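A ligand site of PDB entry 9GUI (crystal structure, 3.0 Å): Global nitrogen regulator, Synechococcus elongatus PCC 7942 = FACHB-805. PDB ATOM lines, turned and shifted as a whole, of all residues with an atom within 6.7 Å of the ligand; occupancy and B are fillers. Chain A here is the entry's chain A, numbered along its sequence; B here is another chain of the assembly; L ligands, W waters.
NH2 of Arg 128 lies within salt-bridge range of OE2 of Glu 133 of chain B, 3.0 Å away.
O of Val 73 sits at hydrogen-bond distance from NH1 of Arg 128, 2.6 Å away.
OG1 of Thr 132 sits at hydrogen-bond distance from O of Arg 128 (2.6 Å).
The backbone carbonyl oxygen (O) of Gly 75 lies within hydrogen-bond range of the side-chain hydroxyl (OG) of Ser 78, at 2.6 Å.
N of Leu 53 is in hydrogen-bond range of O of Ala 66.
The backbone NH (N) of Val 65 sits at hydrogen-bond distance from the backbone carbonyl oxygen (O) of Leu 53, at 2.7 Å.
The backbone carbonyl oxygen (O) of Phe 74 is in hydrogen-bond range of the backbone NH (N) of Tyr 44, 3.0 Å away.
The backbone carbonyl oxygen of Phe 34 is in hydrogen-bond range of the backbone NH of Ala 91 (3.0 Å).
An oxygen (O2) of the ligand is in salt-bridge range of the guanidinium group (NH2) of Arg 128.
The side-chain carboxylate of Glu 133 of chain B sits close to an oxygen (O2) of the ligand (2.7 Å).
O4 of the ligand sits at hydrogen-bond distance from N of Leu 77 (2.8 Å).
O1 of the ligand is in hydrogen-bond range of N of Gly 75 (3.0 Å).
The backbone NH (N) of Val 76 lies within hydrogen-bond range of an oxygen (O4) of the ligand, at 3.0 Å.
The guanidinium group (NE) of Arg 87 lies within salt-bridge range of an oxygen (O5) of the ligand.
Water W1 lies within hydrogen-bond range of an oxygen (O5) of the ligand (2.5 Å), the backbone NH of Phe 88 (2.7 Å) and the backbone NH of Tyr 89 (3.1 Å).
CZ of Phe 34 touches O3 of the ligand, at 3.6 Å.
CD1 of Leu 53 touches O2 of the ligand, 3.3 Å away.
CA of Phe 74 touches O1 of the ligand, 3.5 Å away.
Tyr 89 touches the ligand.
Ile 129 of chain B touches the ligand (CG2 to O2, 3.96 Å).
Leu 130 of chain B touches the ligand (CD2 to C3, 3.4 Å).
Hydrophobic or aromatic side chains within 4 Å of the ligand: Phe 34, Leu 53, Phe 74, Val 76, Leu 77, Tyr 89, Ile 129 of chain B and Leu 130 of chain B.
Along chain A the residues within 4 Å of the ligand span positions 34 to 128.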
ATOM      1  N   PHE A  34     -27.366  17.068  35.385  1.00  0.00           N
ATOM      2  CA  PHE A  34     -28.356  17.456  34.387  1.00  0.00           C
ATOM      3  C   PHE A  34     -28.540  16.327  33.370  1.00  0.00           C
ATOM      4  O   PHE A  34     -27.627  15.526  33.131  1.00  0.00           O
ATOM      5  CB  PHE A  34     -28.017  18.810  33.735  1.00  0.00           C
ATOM      6  CG  PHE A  34     -26.668  18.947  33.058  1.00  0.00           C
ATOM      7  CD1 PHE A  34     -26.298  18.128  31.979  1.00  0.00           C
ATOM      8  CD2 PHE A  34     -25.784  19.933  33.458  1.00  0.00           C
ATOM      9  CE1 PHE A  34     -25.063  18.270  31.358  1.00  0.00           C
ATOM     10  CE2 PHE A  34     -24.553  20.089  32.840  1.00  0.00           C
ATOM     11  CZ  PHE A  34     -24.200  19.257  31.799  1.00  0.00           C
ATOM     12  N   ALA A  40     -30.443  24.357  28.688  1.00  0.00           N
ATOM     13  CA  ALA A  40     -29.113  24.838  29.127  1.00  0.00           C
ATOM     14  C   ALA A  40     -29.260  26.262  29.649  1.00  0.00           C
ATOM     15  O   ALA A  40     -28.880  27.188  28.937  1.00  0.00           O
ATOM     16  CB  ALA A  40     -28.154  24.778  27.981  1.00  0.00           C
ATOM     17  N   TYR A  44     -22.206  26.031  35.840  1.00  0.00           N
ATOM     18  CA  TYR A  44     -21.856  25.396  37.098  1.00  0.00           C
ATOM     19  C   TYR A  44     -20.378  25.606  37.382  1.00  0.00           C
ATOM     20  O   TYR A  44     -19.590  25.744  36.463  1.00  0.00           O
ATOM     21  CB  TYR A  44     -22.086  23.882  37.057  1.00  0.00           C
ATOM     22  CG  TYR A  44     -23.488  23.465  36.676  1.00  0.00           C
ATOM     23  CD1 TYR A  44     -23.851  23.331  35.349  1.00  0.00           C
ATOM     24  CD2 TYR A  44     -24.461  23.244  37.643  1.00  0.00           C
ATOM     25  CE1 TYR A  44     -25.123  22.944  34.996  1.00  0.00           C
ATOM     26  CE2 TYR A  44     -25.741  22.852  37.300  1.00  0.00           C
ATOM     27  CZ  TYR A  44     -26.063  22.709  35.973  1.00  0.00           C
ATOM     28  OH  TYR A  44     -27.305  22.325  35.568  1.00  0.00           O
ATOM     29  N   LEU A  53     -19.063  13.812  32.391  1.00  0.00           N
ATOM     30  CA  LEU A  53     -19.885  14.240  31.265  1.00  0.00           C
ATOM     31  C   LEU A  53     -19.912  13.100  30.251  1.00  0.00           C
ATOM     32  O   LEU A  53     -18.843  12.686  29.781  1.00  0.00           O
ATOM     33  CB  LEU A  53     -19.308  15.524  30.671  1.00  0.00           C
ATOM     34  CG  LEU A  53     -19.427  16.763  31.588  1.00  0.00           C
ATOM     35  CD1 LEU A  53     -19.166  18.033  30.810  1.00  0.00           C
ATOM     36  CD2 LEU A  53     -20.810  16.861  32.245  1.00  0.00           C
ATOM     37  N   VAL A  65     -17.075  11.775  27.964  1.00  0.00           N
ATOM     38  CA  VAL A  65     -16.389  12.866  27.294  1.00  0.00           C
ATOM     39  C   VAL A  65     -15.434  13.627  28.217  1.00  0.00           C
ATOM     40  O   VAL A  65     -14.370  14.066  27.773  1.00  0.00           O
ATOM     41  CB  VAL A  65     -17.369  13.862  26.698  1.00  0.00           C
ATOM     42  CG1 VAL A  65     -16.587  14.963  26.022  1.00  0.00           C
ATOM     43  CG2 VAL A  65     -18.329  13.148  25.756  1.00  0.00           C
ATOM     44  N   ALA A  66     -15.852  13.832  29.474  1.00  0.00           N
ATOM     45  CA  ALA A  66     -15.020  14.524  30.432  1.00  0.00           C
ATOM     46  C   ALA A  66     -15.233  13.953  31.832  1.00  0.00           C
ATOM     47  O   ALA A  66     -16.342  13.703  32.276  1.00  0.00           O
ATOM     48  CB  ALA A  66     -15.338  15.989  30.398  1.00  0.00           C
ATOM     49  N   LEU A  68     -14.466  15.710  34.899  1.00  0.00           N
ATOM     50  CA  LEU A  68     -14.044  17.060  35.261  1.00  0.00           C
ATOM     51  C   LEU A  68     -13.453  17.043  36.660  1.00  0.00           C
ATOM     52  O   LEU A  68     -13.923  16.292  37.492  1.00  0.00           O
ATOM     53  CB  LEU A  68     -15.235  18.022  35.252  1.00  0.00           C
ATOM     54  CG  LEU A  68     -16.013  18.204  33.949  1.00  0.00           C
ATOM     55  CD1 LEU A  68     -17.207  19.108  34.206  1.00  0.00           C
ATOM     56  CD2 LEU A  68     -15.155  18.790  32.845  1.00  0.00           C
ATOM     57  N   VAL A  73     -15.230  24.771  35.632  1.00  0.00           N
ATOM     58  CA  VAL A  73     -16.439  25.384  35.118  1.00  0.00           C
ATOM     59  C   VAL A  73     -17.033  24.433  34.099  1.00  0.00           C
ATOM     60  O   VAL A  73     -16.323  24.022  33.194  1.00  0.00           O
ATOM     61  CB  VAL A  73     -16.160  26.734  34.427  1.00  0.00           C
ATOM     62  CG1 VAL A  73     -17.431  27.334  33.833  1.00  0.00           C
ATOM     63  CG2 VAL A  73     -15.458  27.721  35.357  1.00  0.00           C
ATOM     64  N   PHE A  74     -18.329  24.139  34.211  1.00  0.00           N
ATOM     65  CA  PHE A  74     -18.955  23.367  33.149  1.00  0.00           C
ATOM     66  C   PHE A  74     -20.398  23.827  32.928  1.00  0.00           C
ATOM     67  O   PHE A  74     -20.838  24.847  33.456  1.00  0.00           O
ATOM     68  CB  PHE A  74     -18.842  21.882  33.462  1.00  0.00           C
ATOM     69  CG  PHE A  74     -19.569  21.418  34.701  1.00  0.00           C
ATOM     70  CD1 PHE A  74     -19.072  21.665  35.972  1.00  0.00           C
ATOM     71  CD2 PHE A  74     -20.760  20.728  34.608  1.00  0.00           C
ATOM     72  CE1 PHE A  74     -19.755  21.242  37.103  1.00  0.00           C
ATOM     73  CE2 PHE A  74     -21.434  20.316  35.742  1.00  0.00           C
ATOM     74  CZ  PHE A  74     -20.932  20.584  36.988  1.00  0.00           C
ATOM     75  N   GLY A  75     -21.117  23.120  32.041  1.00  0.00           N
ATOM     76  CA  GLY A  75     -22.451  23.622  31.666  1.00  0.00           C
ATOM     77  C   GLY A  75     -22.259  24.847  30.807  1.00  0.00           C
ATOM     78  O   GLY A  75     -22.929  25.859  31.061  1.00  0.00           O
ATOM     79  N   VAL A  76     -21.410  24.744  29.784  1.00  0.00           N
ATOM     80  CA  VAL A  76     -21.014  25.940  28.985  1.00  0.00           C
ATOM     81  C   VAL A  76     -21.899  26.128  27.745  1.00  0.00           C
ATOM     82  O   VAL A  76     -21.799  27.189  27.120  1.00  0.00           O
ATOM     83  CB  VAL A  76     -19.522  25.794  28.616  1.00  0.00           C
ATOM     84  CG1 VAL A  76     -19.318  25.088  27.289  1.00  0.00           C
ATOM     85  CG2 VAL A  76     -18.797  27.120  28.653  1.00  0.00           C
ATOM     86  N   LEU A  77     -22.737  25.152  27.413  1.00  0.00           N
ATOM     87  CA  LEU A  77     -23.677  25.347  26.285  1.00  0.00           C
ATOM     88  C   LEU A  77     -24.590  26.529  26.623  1.00  0.00           C
ATOM     89  O   LEU A  77     -24.997  27.250  25.697  1.00  0.00           O
ATOM     90  CB  LEU A  77     -24.474  24.059  26.076  1.00  0.00           C
ATOM     91  CG  LEU A  77     -25.550  24.098  24.983  1.00  0.00           C
ATOM     92  CD1 LEU A  77     -24.908  24.056  23.600  1.00  0.00           C
ATOM     93  CD2 LEU A  77     -26.505  22.929  25.157  1.00  0.00           C
ATOM     94  N   SER A  78     -24.876  26.741  27.909  1.00  0.00           N
ATOM     95  CA  SER A  78     -25.692  27.900  28.340  1.00  0.00           C
ATOM     96  C   SER A  78     -24.958  29.190  27.982  1.00  0.00           C
ATOM     97  O   SER A  78     -25.583  30.088  27.390  1.00  0.00           O
ATOM     98  CB  SER A  78     -25.956  27.843  29.809  1.00  0.00           C
ATOM     99  OG  SER A  78     -24.743  27.692  30.526  1.00  0.00           O
ATOM    100  N   ASP A  86     -30.756  22.951  24.275  1.00  0.00           N
ATOM    101  CA  ASP A  86     -31.083  21.984  25.340  1.00  0.00           C
ATOM    102  C   ASP A  86     -29.850  21.101  25.565  1.00  0.00           C
ATOM    103  O   ASP A  86     -29.060  20.957  24.621  1.00  0.00           O
ATOM    104  CB  ASP A  86     -32.351  21.191  24.983  1.00  0.00           C
ATOM    105  CG  ASP A  86     -33.627  21.988  25.186  1.00  0.00           C
ATOM    106  OD1 ASP A  86     -33.535  23.158  25.584  1.00  0.00           O
ATOM    107  OD2 ASP A  86     -34.715  21.411  24.949  1.00  0.00           O
ATOM    108  N   ARG A  87     -29.706  20.553  26.769  1.00  0.00           N
ATOM    109  CA  ARG A  87     -28.507  19.737  27.101  1.00  0.00           C
ATOM    110  C   ARG A  87     -28.489  18.470  26.246  1.00  0.00           C
ATOM    111  O   ARG A  87     -29.564  17.883  26.043  1.00  0.00           O
ATOM    112  CB  ARG A  87     -28.514  19.375  28.590  1.00  0.00           C
ATOM    113  CG  ARG A  87     -27.341  19.946  29.370  1.00  0.00           C
ATOM    114  CD  ARG A  87     -27.314  21.462  29.416  1.00  0.00           C
ATOM    115  NE  ARG A  87     -26.203  21.947  30.225  1.00  0.00           N
ATOM    116  CZ  ARG A  87     -25.922  23.226  30.439  1.00  0.00           C
ATOM    117  NH1 ARG A  87     -26.299  23.818  31.556  1.00  0.00           N
ATOM    118  NH2 ARG A  87     -25.256  23.920  29.526  1.00  0.00           N
ATOM    119  N   PHE A  88     -27.306  18.080  25.761  1.00  0.00           N
ATOM    120  CA  PHE A  88     -27.175  16.822  25.005  1.00  0.00           C
ATOM    121  C   PHE A  88     -26.274  15.796  25.669  1.00  0.00           C
ATOM    122  O   PHE A  88     -26.263  14.635  25.241  1.00  0.00           O
ATOM    123  CB  PHE A  88     -26.658  17.034  23.581  1.00  0.00           C
ATOM    124  CG  PHE A  88     -25.546  18.031  23.424  1.00  0.00           C
ATOM    125  CD1 PHE A  88     -24.240  17.668  23.696  1.00  0.00           C
ATOM    126  CD2 PHE A  88     -25.791  19.323  22.993  1.00  0.00           C
ATOM    127  CE1 PHE A  88     -23.206  18.575  23.526  1.00  0.00           C
ATOM    128  CE2 PHE A  88     -24.757  20.229  22.823  1.00  0.00           C
ATOM    129  CZ  PHE A  88     -23.478  19.845  23.083  1.00  0.00           C
ATOM    130  N   TYR A  89     -25.534  16.204  26.698  1.00  0.00           N
ATOM    131  CA  TYR A  89     -24.761  15.278  27.495  1.00  0.00           C
ATOM    132  C   TYR A  89     -25.424  15.059  28.861  1.00  0.00           C
ATOM    133  O   TYR A  89     -26.309  15.817  29.263  1.00  0.00           O
ATOM    134  CB  TYR A  89     -23.346  15.795  27.684  1.00  0.00           C
ATOM    135  CG  TYR A  89     -22.455  15.854  26.471  1.00  0.00           C
ATOM    136  CD1 TYR A  89     -22.455  14.865  25.505  1.00  0.00           C
ATOM    137  CD2 TYR A  89     -21.560  16.884  26.332  1.00  0.00           C
ATOM    138  CE1 TYR A  89     -21.610  14.941  24.405  1.00  0.00           C
ATOM    139  CE2 TYR A  89     -20.700  16.963  25.245  1.00  0.00           C
ATOM    140  CZ  TYR A  89     -20.725  15.988  24.275  1.00  0.00           C
ATOM    141  OH  TYR A  89     -19.826  16.141  23.222  1.00  0.00           O
ATOM    142  N   ALA A  91     -24.709  14.922  32.737  1.00  0.00           N
ATOM    143  CA  ALA A  91     -23.756  15.307  33.768  1.00  0.00           C
ATOM    144  C   ALA A  91     -24.075  14.531  35.035  1.00  0.00           C
ATOM    145  O   ALA A  91     -25.183  14.636  35.520  1.00  0.00           O
ATOM    146  CB  ALA A  91     -23.812  16.794  34.029  1.00  0.00           C
ATOM    147  N   ARG A 128     -10.376  24.574  30.394  1.00  0.00           N
ATOM    148  CA  ARG A 128     -11.216  23.469  29.902  1.00  0.00           C
ATOM    149  C   ARG A 128     -10.747  23.042  28.503  1.00  0.00           C
ATOM    150  O   ARG A 128     -10.583  21.846  28.244  1.00  0.00           O
ATOM    151  CB  ARG A 128     -12.695  23.886  29.889  1.00  0.00           C
ATOM    152  CG  ARG A 128     -13.333  24.045  31.259  1.00  0.00           C
ATOM    153  CD  ARG A 128     -13.546  22.730  31.959  1.00  0.00           C
ATOM    154  NE  ARG A 128     -14.088  21.709  31.081  1.00  0.00           N
ATOM    155  CZ  ARG A 128     -15.357  21.630  30.694  1.00  0.00           C
ATOM    156  NH1 ARG A 128     -16.236  22.541  31.092  1.00  0.00           N
ATOM    157  NH2 ARG A 128     -15.746  20.640  29.910  1.00  0.00           N
ATOM    158  N   THR A 132      -9.328  19.420  27.602  1.00  0.00           N
ATOM    159  CA  THR A 132     -10.052  18.557  26.690  1.00  0.00           C
ATOM    160  C   THR A 132      -9.126  18.090  25.569  1.00  0.00           C
ATOM    161  O   THR A 132      -9.217  16.959  25.131  1.00  0.00           O
ATOM    162  CB  THR A 132     -11.293  19.261  26.117  1.00  0.00           C
ATOM    163  OG1 THR A 132     -11.998  19.909  27.175  1.00  0.00           O
ATOM    164  CG2 THR A 132     -12.218  18.336  25.363  1.00  0.00           C
ATOM    165  N   ILE B 129     -14.829  24.384  23.494  1.00  0.00           N
ATOM    166  CA  ILE B 129     -14.934  23.253  24.451  1.00  0.00           C
ATOM    167  C   ILE B 129     -15.876  22.210  23.850  1.00  0.00           C
ATOM    168  O   ILE B 129     -15.518  21.027  23.812  1.00  0.00           O
ATOM    169  CB  ILE B 129     -15.440  23.740  25.820  1.00  0.00           C
ATOM    170  CG1 ILE B 129     -14.523  24.798  26.417  1.00  0.00           C
ATOM    171  CG2 ILE B 129     -15.640  22.571  26.773  1.00  0.00           C
ATOM    172  CD1 ILE B 129     -15.078  25.461  27.654  1.00  0.00           C
ATOM    173  N   LEU B 130     -17.051  22.653  23.375  1.00  0.00           N
ATOM    174  CA  LEU B 130     -18.065  21.707  22.856  1.00  0.00           C
ATOM    175  C   LEU B 130     -17.543  21.025  21.585  1.00  0.00           C
ATOM    176  O   LEU B 130     -17.763  19.823  21.424  1.00  0.00           O
ATOM    177  CB  LEU B 130     -19.349  22.492  22.585  1.00  0.00           C
ATOM    178  CG  LEU B 130     -19.998  23.126  23.813  1.00  0.00           C
ATOM    179  CD1 LEU B 130     -21.277  23.844  23.424  1.00  0.00           C
ATOM    180  CD2 LEU B 130     -20.271  22.079  24.876  1.00  0.00           C
ATOM    181  N   GLU B 133     -14.943  18.475  22.593  1.00  0.00           N
ATOM    182  CA  GLU B 133     -15.622  17.319  23.173  1.00  0.00           C
ATOM    183  C   GLU B 133     -16.218  16.426  22.083  1.00  0.00           C
ATOM    184  O   GLU B 133     -16.008  15.224  22.054  1.00  0.00           O
ATOM    185  CB  GLU B 133     -16.690  17.774  24.152  1.00  0.00           C
ATOM    186  CG  GLU B 133     -16.111  18.258  25.467  1.00  0.00           C
ATOM    187  CD  GLU B 133     -17.096  18.827  26.466  1.00  0.00           C
ATOM    188  OE1 GLU B 133     -18.244  19.185  26.086  1.00  0.00           O
ATOM    189  OE2 GLU B 133     -16.708  18.912  27.649  1.00  0.00           O
HETATM  190  C1  LIG L   1     -19.245  21.260  29.299  1.00  0.00           C
HETATM  191  O1  LIG L   1     -19.264  22.382  29.761  1.00  0.00           O
HETATM  192  O2  LIG L   1     -18.215  20.624  29.061  1.00  0.00           O
HETATM  193  C2  LIG L   1     -20.508  20.612  29.066  1.00  0.00           C
HETATM  194  O3  LIG L   1     -21.320  20.338  29.945  1.00  0.00           O
HETATM  195  C3  LIG L   1     -20.819  20.265  27.639  1.00  0.00           C
HETATM  196  C4  LIG L   1     -22.313  20.170  27.477  1.00  0.00           C
HETATM  197  C5  LIG L   1     -23.092  21.430  27.829  1.00  0.00           C
HETATM  198  O4  LIG L   1     -22.464  22.481  28.051  1.00  0.00           O
HETATM  199  O5  LIG L   1     -24.336  21.342  27.901  1.00  0.00           O
HETATM  200  O   HOH W   1     -25.054  19.289  26.714  1.00  0.00           O
